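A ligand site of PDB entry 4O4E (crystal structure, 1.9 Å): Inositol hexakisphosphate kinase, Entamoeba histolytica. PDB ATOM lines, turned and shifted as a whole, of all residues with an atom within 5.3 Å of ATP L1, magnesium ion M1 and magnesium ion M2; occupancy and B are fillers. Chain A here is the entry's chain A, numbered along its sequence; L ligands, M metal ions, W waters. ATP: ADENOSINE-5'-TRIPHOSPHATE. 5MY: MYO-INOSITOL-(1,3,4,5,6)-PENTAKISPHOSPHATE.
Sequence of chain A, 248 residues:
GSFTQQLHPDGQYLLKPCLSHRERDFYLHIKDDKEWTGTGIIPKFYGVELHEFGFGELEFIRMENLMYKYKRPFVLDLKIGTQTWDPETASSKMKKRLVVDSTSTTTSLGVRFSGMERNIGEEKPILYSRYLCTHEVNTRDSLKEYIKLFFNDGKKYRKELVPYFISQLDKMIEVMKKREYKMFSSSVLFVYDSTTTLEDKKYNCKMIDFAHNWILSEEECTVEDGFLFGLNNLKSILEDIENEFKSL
Magnesium ion M1 is bound by O1B of ATP L1, 2.0 Å away. Water W7 is bound to magnesium ion M1, at 2.1 Å. Magnesium ion M1 is bound by water W9 (2.1 Å). Water W5 binds magnesium ion M1 (2.1 Å). Magnesium ion M1 is bound by an oxygen (O34) of 5MY L2 (2.2 Å). Magnesium ion M1 is bound by O2G of ATP L1 (2.3 Å).
Merely in contact with ATP L1: Phe 3, Leu 14, Asn 65, Leu 189, Ile 208 and Ala 211. Hydrophobic or aromatic side chains that line ATP L1: Phe 3, Leu 14, Met 63, Leu 66, Leu 189, Ile 208 and Ala 211. Of the 21 residues printed, 15 come within 4 Å of ATP L1.
Gly 1 touches magnesium ion M1 (N to MG, 3.6 Å). Of the 21 residues printed, 1 comes within 4 Å of magnesium ion M1.
The backbone NH of Ser 2 lies within hydrogen-bond range of an oxygen (O2B) of ATP L1 (2.8 Å). OG of Ser 2 is in hydrogen-bond range of O2B of ATP L1, 2.6 Å away. The side-chain amino group (NZ) of Lys 16 is in salt-bridge range of an oxygen (O1A) of ATP L1, at 2.8 Å. O2B of ATP L1 lies within hydrogen-bond range of N of Gly 1 (3.2 Å). O of Glu 64 lies within hydrogen-bond range of N6 of ATP L1 (2.9 Å). The backbone NH of Leu 66 is in hydrogen-bond range of a nitrogen (N1) of ATP L1. The side-chain carboxylate (OD2) of Asp 77 is in hydrogen-bond range of an oxygen (O3') of ATP L1, 3.3 Å away. The side-chain amide nitrogen of Gln 5 sits close to an oxygen (O1B) of ATP L1 (3.5 Å). SD of Met 63 is in hydrogen-bond range of N6 of ATP L1 (3.6 Å). N of Gly 1 sits close to O24 of 5MY L2 (3.5 Å). The side-chain amide nitrogen (NE2) of Gln 5 lies close to an oxygen (O34) of 5MY L2 (3.0 Å).
Water W9 bridges an oxygen (O33) of 5MY L2 (2.8 Å) and the backbone NH (N) of Gly 1 (3.4 Å). Water W4 bridges an oxygen (O35) of 5MY L2 (3.1 Å) and the backbone carbonyl oxygen (O) of Ser 185 (3.2 Å). Water W2 lies within hydrogen-bond range of O1A of ATP L1 (2.8 Å) and SD of Met 63 (3.8 Å). Water W8 lies within hydrogen-bond range of an oxygen (O2A) of ATP L1 (2.9 Å) and the side-chain carboxylate of Asp 77 (3.3 Å).
OD1 of Asp 209 is in salt-bridge range of NZ of Lys 16 (3.5 Å). NZ of Lys 16 lies within salt-bridge range of OE1 of Glu 23 (2.7 Å). NE2 of Gln 5 sits close to N of Gly 1. The side-chain amide oxygen (OD1) of Asn 65 is in hydrogen-bond range of the backbone NH (N) of Met 67 (3.0 Å). O of Met 63 is in hydrogen-bond range of N of Leu 14 (2.9 Å).
Magnesium ion M2 is bound by an oxygen (O2G) of ATP L1 (2.0 Å), the side-chain carboxylate of Asp 209 (2.2 Å), water W5 (2.2 Å), water W4 (2.5 Å) and water W1 (2.5 Å). Magnesium ion M2 has five donor atoms within binding distance. Slightly farther from magnesium ion M2 lies water W7 (2.7 Å).
Of the 21 residues printed, 1 comes within 4 Å of magnesium ion M2.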
ATOM      1  N   GLY A   1      -5.672 -20.477  -8.759  1.00  0.00           N
ATOM      2  CA  GLY A   1      -5.002 -20.193  -7.467  1.00  0.00           C
ATOM      3  C   GLY A   1      -3.717 -19.405  -7.622  1.00  0.00           C
ATOM      4  O   GLY A   1      -3.388 -18.616  -6.753  1.00  0.00           O
ATOM      5  N   SER A   2      -2.968 -19.616  -8.705  1.00  0.00           N
ATOM      6  CA  SER A   2      -1.643 -18.983  -8.819  1.00  0.00           C
ATOM      7  C   SER A   2      -1.697 -17.546  -9.379  1.00  0.00           C
ATOM      8  O   SER A   2      -0.678 -16.861  -9.396  1.00  0.00           O
ATOM      9  CB  SER A   2      -0.704 -19.860  -9.639  1.00  0.00           C
ATOM     10  OG  SER A   2      -1.129 -20.002 -10.977  1.00  0.00           O
ATOM     11  N   PHE A   3      -2.876 -17.101  -9.840  1.00  0.00           N
ATOM     12  CA  PHE A   3      -3.096 -15.722 -10.320  1.00  0.00           C
ATOM     13  C   PHE A   3      -4.557 -15.306 -10.036  1.00  0.00           C
ATOM     14  O   PHE A   3      -5.427 -16.182  -9.899  1.00  0.00           O
ATOM     15  CB  PHE A   3      -2.785 -15.614 -11.846  1.00  0.00           C
ATOM     16  CG  PHE A   3      -3.546 -16.623 -12.697  1.00  0.00           C
ATOM     17  CD1 PHE A   3      -4.845 -16.354 -13.131  1.00  0.00           C
ATOM     18  CD2 PHE A   3      -2.993 -17.858 -13.037  1.00  0.00           C
ATOM     19  CE1 PHE A   3      -5.554 -17.273 -13.877  1.00  0.00           C
ATOM     20  CE2 PHE A   3      -3.701 -18.785 -13.789  1.00  0.00           C
ATOM     21  CZ  PHE A   3      -4.977 -18.485 -14.226  1.00  0.00           C
ATOM     22  N   GLN A   5      -8.029 -14.856 -10.797  1.00  0.00           N
ATOM     23  CA  GLN A   5      -8.635 -15.681 -11.859  1.00  0.00           C
ATOM     24  C   GLN A   5      -9.542 -14.962 -12.842  1.00  0.00           C
ATOM     25  O   GLN A   5      -9.967 -15.566 -13.848  1.00  0.00           O
ATOM     26  CB  GLN A   5      -9.371 -16.890 -11.257  1.00  0.00           C
ATOM     27  CG  GLN A   5      -8.421 -17.879 -10.609  1.00  0.00           C
ATOM     28  CD  GLN A   5      -9.047 -19.244 -10.361  1.00  0.00           C
ATOM     29  OE1 GLN A   5     -10.270 -19.358 -10.244  1.00  0.00           O
ATOM     30  NE2 GLN A   5      -8.208 -20.279 -10.275  1.00  0.00           N
ATOM     31  N   PRO A   9     -10.931 -10.989 -17.824  1.00  0.00           N
ATOM     32  CA  PRO A   9     -10.030 -11.194 -18.940  1.00  0.00           C
ATOM     33  C   PRO A   9     -10.435 -10.417 -20.212  1.00  0.00           C
ATOM     34  O   PRO A   9     -11.315 -10.854 -20.965  1.00  0.00           O
ATOM     35  CB  PRO A   9     -10.080 -12.718 -19.133  1.00  0.00           C
ATOM     36  CG  PRO A   9     -10.305 -13.258 -17.775  1.00  0.00           C
ATOM     37  CD  PRO A   9     -11.099 -12.225 -17.034  1.00  0.00           C
ATOM     38  N   LEU A  14      -2.583 -14.614 -21.116  1.00  0.00           N
ATOM     39  CA  LEU A  14      -2.475 -15.064 -19.739  1.00  0.00           C
ATOM     40  C   LEU A  14      -1.015 -15.392 -19.548  1.00  0.00           C
ATOM     41  O   LEU A  14      -0.443 -16.158 -20.305  1.00  0.00           O
ATOM     42  CB  LEU A  14      -3.313 -16.326 -19.510  1.00  0.00           C
ATOM     43  CG  LEU A  14      -3.121 -17.084 -18.198  1.00  0.00           C
ATOM     44  CD1 LEU A  14      -3.393 -16.158 -17.011  1.00  0.00           C
ATOM     45  CD2 LEU A  14      -4.021 -18.299 -18.104  1.00  0.00           C
ATOM     46  N   LYS A  16       1.022 -17.191 -17.020  1.00  0.00           N
ATOM     47  CA  LYS A  16       0.812 -18.118 -15.881  1.00  0.00           C
ATOM     48  C   LYS A  16       2.144 -18.580 -15.310  1.00  0.00           C
ATOM     49  O   LYS A  16       3.000 -19.070 -16.050  1.00  0.00           O
ATOM     50  CB  LYS A  16       0.012 -19.335 -16.357  1.00  0.00           C
ATOM     51  CG  LYS A  16      -0.431 -20.256 -15.230  1.00  0.00           C
ATOM     52  CD  LYS A  16      -1.165 -21.497 -15.730  1.00  0.00           C
ATOM     53  CE  LYS A  16      -1.352 -22.483 -14.577  1.00  0.00           C
ATOM     54  NZ  LYS A  16      -2.167 -23.634 -15.025  1.00  0.00           N
ATOM     55  N   GLU A  23       3.570 -28.570 -16.229  1.00  0.00           N
ATOM     56  CA  GLU A  23       2.774 -27.851 -17.242  1.00  0.00           C
ATOM     57  C   GLU A  23       3.700 -27.390 -18.342  1.00  0.00           C
ATOM     58  O   GLU A  23       3.420 -27.592 -19.531  1.00  0.00           O
ATOM     59  CB  GLU A  23       1.983 -26.665 -16.632  1.00  0.00           C
ATOM     60  CG  GLU A  23       1.062 -25.961 -17.646  1.00  0.00           C
ATOM     61  CD  GLU A  23      -0.078 -25.216 -16.967  1.00  0.00           C
ATOM     62  OE1 GLU A  23       0.221 -24.478 -15.987  1.00  0.00           O
ATOM     63  OE2 GLU A  23      -1.260 -25.428 -17.353  1.00  0.00           O
ATOM     64  N   PRO A  43      -5.028 -23.897 -25.508  1.00  0.00           N
ATOM     65  CA  PRO A  43      -4.717 -22.497 -25.800  1.00  0.00           C
ATOM     66  C   PRO A  43      -3.432 -22.325 -26.636  1.00  0.00           C
ATOM     67  O   PRO A  43      -2.504 -23.140 -26.556  1.00  0.00           O
ATOM     68  CB  PRO A  43      -4.546 -21.897 -24.403  1.00  0.00           C
ATOM     69  CG  PRO A  43      -5.341 -22.811 -23.535  1.00  0.00           C
ATOM     70  CD  PRO A  43      -5.030 -24.161 -24.075  1.00  0.00           C
ATOM     71  N   MET A  63       0.338 -17.698 -22.798  1.00  0.00           N
ATOM     72  CA  MET A  63      -0.694 -18.275 -23.642  1.00  0.00           C
ATOM     73  C   MET A  63      -1.773 -17.268 -23.974  1.00  0.00           C
ATOM     74  O   MET A  63      -1.842 -16.190 -23.390  1.00  0.00           O
ATOM     75  CB  MET A  63      -1.242 -19.546 -22.980  1.00  0.00           C
ATOM     76  CG  MET A  63      -2.312 -19.336 -21.963  1.00  0.00           C
ATOM     77  SD  MET A  63      -2.748 -20.868 -21.079  1.00  0.00           S
ATOM     78  CE  MET A  63      -1.392 -21.136 -19.968  1.00  0.00           C
ATOM     79  N   GLU A  64      -2.615 -17.603 -24.951  1.00  0.00           N
ATOM     80  CA  GLU A  64      -3.744 -16.742 -25.283  1.00  0.00           C
ATOM     81  C   GLU A  64      -4.758 -16.694 -24.131  1.00  0.00           C
ATOM     82  O   GLU A  64      -5.020 -17.713 -23.471  1.00  0.00           O
ATOM     83  CB  GLU A  64      -4.434 -17.187 -26.601  1.00  0.00           C
ATOM     84  CG  GLU A  64      -5.405 -18.347 -26.459  1.00  0.00           C
ATOM     85  CD  GLU A  64      -6.083 -18.837 -27.749  1.00  0.00           C
ATOM     86  OE1 GLU A  64      -5.822 -19.994 -28.153  1.00  0.00           O
ATOM     87  OE2 GLU A  64      -6.869 -18.088 -28.359  1.00  0.00           O
ATOM     88  N   ASN A  65      -5.317 -15.513 -23.920  1.00  0.00           N
ATOM     89  CA  ASN A  65      -6.526 -15.353 -23.122  1.00  0.00           C
ATOM     90  C   ASN A  65      -7.727 -15.728 -23.988  1.00  0.00           C
ATOM     91  O   ASN A  65      -8.020 -15.032 -24.976  1.00  0.00           O
ATOM     92  CB  ASN A  65      -6.669 -13.902 -22.685  1.00  0.00           C
ATOM     93  CG  ASN A  65      -7.953 -13.637 -21.919  1.00  0.00           C
ATOM     94  OD1 ASN A  65      -8.722 -14.552 -21.569  1.00  0.00           O
ATOM     95  ND2 ASN A  65      -8.201 -12.370 -21.655  1.00  0.00           N
ATOM     96  N   LEU A  66      -8.384 -16.835 -23.619  1.00  0.00           N
ATOM     97  CA  LEU A  66      -9.515 -17.358 -24.400  1.00  0.00           C
ATOM     98  C   LEU A  66     -10.731 -16.447 -24.467  1.00  0.00           C
ATOM     99  O   LEU A  66     -11.579 -16.602 -25.365  1.00  0.00           O
ATOM    100  CB  LEU A  66      -9.928 -18.763 -23.889  1.00  0.00           C
ATOM    101  CG  LEU A  66      -8.834 -19.819 -23.932  1.00  0.00           C
ATOM    102  CD1 LEU A  66      -9.264 -21.072 -23.209  1.00  0.00           C
ATOM    103  CD2 LEU A  66      -8.434 -20.099 -25.356  1.00  0.00           C
ATOM    104  N   MET A  67     -10.832 -15.474 -23.558  1.00  0.00           N
ATOM    105  CA  MET A  67     -11.935 -14.524 -23.560  1.00  0.00           C
ATOM    106  C   MET A  67     -11.564 -13.091 -23.951  1.00  0.00           C
ATOM    107  O   MET A  67     -12.326 -12.172 -23.680  1.00  0.00           O
ATOM    108  CB  MET A  67     -12.600 -14.540 -22.190  1.00  0.00           C
ATOM    109  CG  MET A  67     -13.291 -15.868 -21.936  1.00  0.00           C
ATOM    110  SD  MET A  67     -14.054 -15.895 -20.338  1.00  0.00           S
ATOM    111  CE  MET A  67     -12.663 -16.323 -19.294  1.00  0.00           C
ATOM    112  N   VAL A  75     -18.907 -18.793 -19.016  1.00  0.00           N
ATOM    113  CA  VAL A  75     -17.768 -19.714 -18.719  1.00  0.00           C
ATOM    114  C   VAL A  75     -18.249 -20.916 -17.922  1.00  0.00           C
ATOM    115  O   VAL A  75     -18.948 -20.741 -16.901  1.00  0.00           O
ATOM    116  CB  VAL A  75     -16.709 -19.021 -17.872  1.00  0.00           C
ATOM    117  CG1 VAL A  75     -15.434 -19.889 -17.737  1.00  0.00           C
ATOM    118  CG2 VAL A  75     -16.378 -17.662 -18.469  1.00  0.00           C
ATOM    119  N   ASP A  77     -16.437 -24.575 -16.460  1.00  0.00           N
ATOM    120  CA  ASP A  77     -15.248 -25.398 -16.264  1.00  0.00           C
ATOM    121  C   ASP A  77     -15.686 -26.781 -15.817  1.00  0.00           C
ATOM    122  O   ASP A  77     -16.378 -26.919 -14.786  1.00  0.00           O
ATOM    123  CB  ASP A  77     -14.339 -24.767 -15.200  1.00  0.00           C
ATOM    124  CG  ASP A  77     -13.011 -25.490 -15.094  1.00  0.00           C
ATOM    125  OD1 ASP A  77     -12.988 -26.696 -14.736  1.00  0.00           O
ATOM    126  OD2 ASP A  77     -11.957 -24.867 -15.384  1.00  0.00           O
ATOM    127  N   SER A 185      -6.688 -33.738 -12.924  1.00  0.00           N
ATOM    128  CA  SER A 185      -7.176 -32.445 -12.468  1.00  0.00           C
ATOM    129  C   SER A 185      -7.210 -31.374 -13.569  1.00  0.00           C
ATOM    130  O   SER A 185      -7.477 -30.186 -13.272  1.00  0.00           O
ATOM    131  CB  SER A 185      -6.346 -31.997 -11.231  1.00  0.00           C
ATOM    132  OG  SER A 185      -6.728 -32.758 -10.086  1.00  0.00           O
ATOM    133  N   LEU A 189     -12.590 -26.147 -20.654  1.00  0.00           N
ATOM    134  CA  LEU A 189     -13.226 -24.856 -20.432  1.00  0.00           C
ATOM    135  C   LEU A 189     -14.102 -24.528 -21.659  1.00  0.00           C
ATOM    136  O   LEU A 189     -13.637 -24.591 -22.813  1.00  0.00           O
ATOM    137  CB  LEU A 189     -12.168 -23.776 -20.262  1.00  0.00           C
ATOM    138  CG  LEU A 189     -12.611 -22.384 -19.798  1.00  0.00           C
ATOM    139  CD1 LEU A 189     -13.006 -22.441 -18.365  1.00  0.00           C
ATOM    140  CD2 LEU A 189     -11.488 -21.373 -20.003  1.00  0.00           C
ATOM    141  N   ILE A 208      -7.409 -27.257 -20.609  1.00  0.00           N
ATOM    142  CA  ILE A 208      -6.547 -26.365 -19.853  1.00  0.00           C
ATOM    143  C   ILE A 208      -6.045 -27.044 -18.545  1.00  0.00           C
ATOM    144  O   ILE A 208      -6.578 -28.077 -18.105  1.00  0.00           O
ATOM    145  CB  ILE A 208      -7.225 -25.021 -19.478  1.00  0.00           C
ATOM    146  CG1 ILE A 208      -8.442 -25.270 -18.598  1.00  0.00           C
ATOM    147  CG2 ILE A 208      -7.692 -24.244 -20.694  1.00  0.00           C
ATOM    148  CD1 ILE A 208      -8.830 -24.117 -17.735  1.00  0.00           C
ATOM    149  N   ASP A 209      -5.025 -26.438 -17.954  1.00  0.00           N
ATOM    150  CA  ASP A 209      -4.459 -26.738 -16.632  1.00  0.00           C
ATOM    151  C   ASP A 209      -3.730 -28.060 -16.538  1.00  0.00           C
ATOM    152  O   ASP A 209      -4.307 -29.091 -16.140  1.00  0.00           O
ATOM    153  CB  ASP A 209      -5.512 -26.676 -15.569  1.00  0.00           C
ATOM    154  CG  ASP A 209      -4.922 -26.718 -14.166  1.00  0.00           C
ATOM    155  OD1 ASP A 209      -3.641 -26.604 -13.980  1.00  0.00           O
ATOM    156  OD2 ASP A 209      -5.761 -26.904 -13.257  1.00  0.00           O
ATOM    157  N   ALA A 211      -0.831 -28.811 -14.910  1.00  0.00           N
ATOM    158  CA  ALA A 211       0.116 -28.923 -13.801  1.00  0.00           C
ATOM    159  C   ALA A 211       0.362 -30.354 -13.332  1.00  0.00           C
ATOM    160  O   ALA A 211       1.342 -30.642 -12.646  1.00  0.00           O
ATOM    161  CB  ALA A 211      -0.393 -28.099 -12.650  1.00  0.00           C
HETATM  162  PG  ATP L   1      -3.015 -24.722 -11.118  1.00  0.00           P
HETATM  163  O1G ATP L   1      -2.361 -25.117 -12.420  1.00  0.00           O
HETATM  164  O2G ATP L   1      -4.484 -25.055 -10.970  1.00  0.00           O
HETATM  165  O3G ATP L   1      -2.169 -25.040  -9.908  1.00  0.00           O
HETATM  166  PB  ATP L   1      -4.252 -22.142 -11.450  1.00  0.00           P
HETATM  167  O1B ATP L   1      -5.557 -22.490 -10.783  1.00  0.00           O
HETATM  168  O2B ATP L   1      -3.590 -20.809 -11.193  1.00  0.00           O
HETATM  169  O3B ATP L   1      -3.002 -23.108 -11.160  1.00  0.00           O
HETATM  170  PA  ATP L   1      -5.624 -22.770 -14.060  1.00  0.00           P
HETATM  171  O1A ATP L   1      -4.901 -23.102 -15.351  1.00  0.00           O
HETATM  172  O2A ATP L   1      -6.445 -23.828 -13.388  1.00  0.00           O
HETATM  173  O3A ATP L   1      -4.470 -22.188 -13.075  1.00  0.00           O
HETATM  174  O5' ATP L   1      -6.558 -21.508 -14.388  1.00  0.00           O
HETATM  175  C5' ATP L   1      -7.523 -21.012 -13.443  1.00  0.00           C
HETATM  176  C4' ATP L   1      -8.767 -20.482 -14.169  1.00  0.00           C
HETATM  177  O4' ATP L   1      -8.466 -19.424 -15.087  1.00  0.00           O
HETATM  178  C3' ATP L   1      -9.442 -21.572 -15.001  1.00  0.00           C
HETATM  179  O3' ATP L   1     -10.329 -22.326 -14.157  1.00  0.00           O
HETATM  180  C2' ATP L   1     -10.138 -20.779 -16.077  1.00  0.00           C
HETATM  181  O2' ATP L   1     -11.363 -20.238 -15.608  1.00  0.00           O
HETATM  182  C1' ATP L   1      -9.236 -19.591 -16.284  1.00  0.00           C
HETATM  183  N9  ATP L   1      -8.273 -19.840 -17.382  1.00  0.00           N
HETATM  184  C8  ATP L   1      -7.240 -20.701 -17.374  1.00  0.00           C
HETATM  185  N7  ATP L   1      -6.574 -20.663 -18.543  1.00  0.00           N
HETATM  186  C5  ATP L   1      -7.214 -19.702 -19.287  1.00  0.00           C
HETATM  187  C6  ATP L   1      -7.021 -19.063 -20.599  1.00  0.00           C
HETATM  188  N6  ATP L   1      -6.038 -19.471 -21.409  1.00  0.00           N
HETATM  189  N1  ATP L   1      -7.879 -18.121 -20.994  1.00  0.00           N
HETATM  190  C2  ATP L   1      -8.906 -17.711 -20.227  1.00  0.00           C
HETATM  191  N3  ATP L   1      -9.133 -18.220 -19.004  1.00  0.00           N
HETATM  192  C4  ATP L   1      -8.319 -19.175 -18.503  1.00  0.00           C
HETATM  193  O31 5MY L   2      -6.477 -27.411  -0.306  1.00  0.00           O
HETATM  194  P1  5MY L   2      -7.092 -28.185  -1.419  1.00  0.00           P
HETATM  195  O21 5MY L   2      -7.974 -29.256  -0.952  1.00  0.00           O
HETATM  196  O41 5MY L   2      -6.170 -28.539  -2.520  1.00  0.00           O
HETATM  197  O11 5MY L   2      -8.143 -27.105  -2.005  1.00  0.00           O
HETATM  198  C1  5MY L   2      -7.913 -26.479  -3.278  1.00  0.00           C
HETATM  199  C2  5MY L   2      -7.338 -25.116  -3.024  1.00  0.00           C
HETATM  200  O12 5MY L   2      -8.293 -24.284  -2.280  1.00  0.00           O
HETATM  201  C3  5MY L   2      -6.969 -24.526  -4.392  1.00  0.00           C
HETATM  202  O13 5MY L   2      -6.333 -23.248  -4.216  1.00  0.00           O
HETATM  203  P3  5MY L   2      -4.701 -23.186  -4.121  1.00  0.00           P
HETATM  204  O23 5MY L   2      -4.371 -21.789  -4.424  1.00  0.00           O
HETATM  205  O33 5MY L   2      -4.186 -24.185  -5.097  1.00  0.00           O
HETATM  206  O43 5MY L   2      -4.536 -23.573  -2.701  1.00  0.00           O
HETATM  207  C6  5MY L   2      -9.176 -26.346  -4.120  1.00  0.00           C
HETATM  208  O16 5MY L   2      -9.769 -27.619  -4.328  1.00  0.00           O
HETATM  209  P6  5MY L   2     -11.350 -27.946  -4.106  1.00  0.00           P
HETATM  210  O26 5MY L   2     -11.980 -27.188  -5.226  1.00  0.00           O
HETATM  211  O36 5MY L   2     -11.239 -29.435  -4.222  1.00  0.00           O
HETATM  212  O46 5MY L   2     -11.459 -27.394  -2.724  1.00  0.00           O
HETATM  213  C5  5MY L   2      -8.793 -25.774  -5.495  1.00  0.00           C
HETATM  214  O15 5MY L   2      -9.994 -25.663  -6.331  1.00  0.00           O
HETATM  215  P5  5MY L   2     -10.183 -26.352  -7.781  1.00  0.00           P
HETATM  216  O25 5MY L   2     -10.606 -25.203  -8.618  1.00  0.00           O
HETATM  217  O35 5MY L   2      -8.869 -26.949  -8.149  1.00  0.00           O
HETATM  218  O45 5MY L   2     -11.294 -27.327  -7.570  1.00  0.00           O
HETATM  219  C4  5MY L   2      -8.174 -24.403  -5.310  1.00  0.00           C
HETATM  220  O14 5MY L   2      -7.717 -23.954  -6.598  1.00  0.00           O
HETATM  221  P4  5MY L   2      -8.289 -22.672  -7.383  1.00  0.00           P
HETATM  222  O34 5MY L   2      -7.509 -22.733  -8.654  1.00  0.00           O
HETATM  223  O44 5MY L   2      -9.742 -22.897  -7.617  1.00  0.00           O
HETATM  224  O24 5MY L   2      -7.974 -21.586  -6.440  1.00  0.00           O
HETATM  225 MG    MG M   1      -5.926 -23.971  -9.497  1.00  0.00          MG
HETATM  226 MG    MG M   2      -5.937 -26.479 -11.135  1.00  0.00          MG
HETATM  227  O   HOH W   1      -4.488 -28.519 -11.053  1.00  0.00           O
HETATM  228  O   HOH W   2      -4.331 -22.429 -18.036  1.00  0.00           O
HETATM  229  O   HOH W   3       0.504 -24.303 -11.072  1.00  0.00           O
HETATM  230  O   HOH W   4      -7.842 -28.050 -10.889  1.00  0.00           O
HETATM  231  O   HOH W   5      -7.142 -24.638 -11.071  1.00  0.00           O
HETATM  232  O   HOH W   6      -5.644 -18.975 -10.696  1.00  0.00           O
HETATM  233  O   HOH W   7      -6.344 -25.774  -8.591  1.00  0.00           O
HETATM  234  O   HOH W   8      -8.841 -25.005 -14.394  1.00  0.00           O
HETATM  235  O   HOH W   9      -4.779 -23.596  -7.806  1.00  0.00           O
HETATM  236  O   HOH W  10      -2.272 -27.437  -9.122  1.00  0.00           O
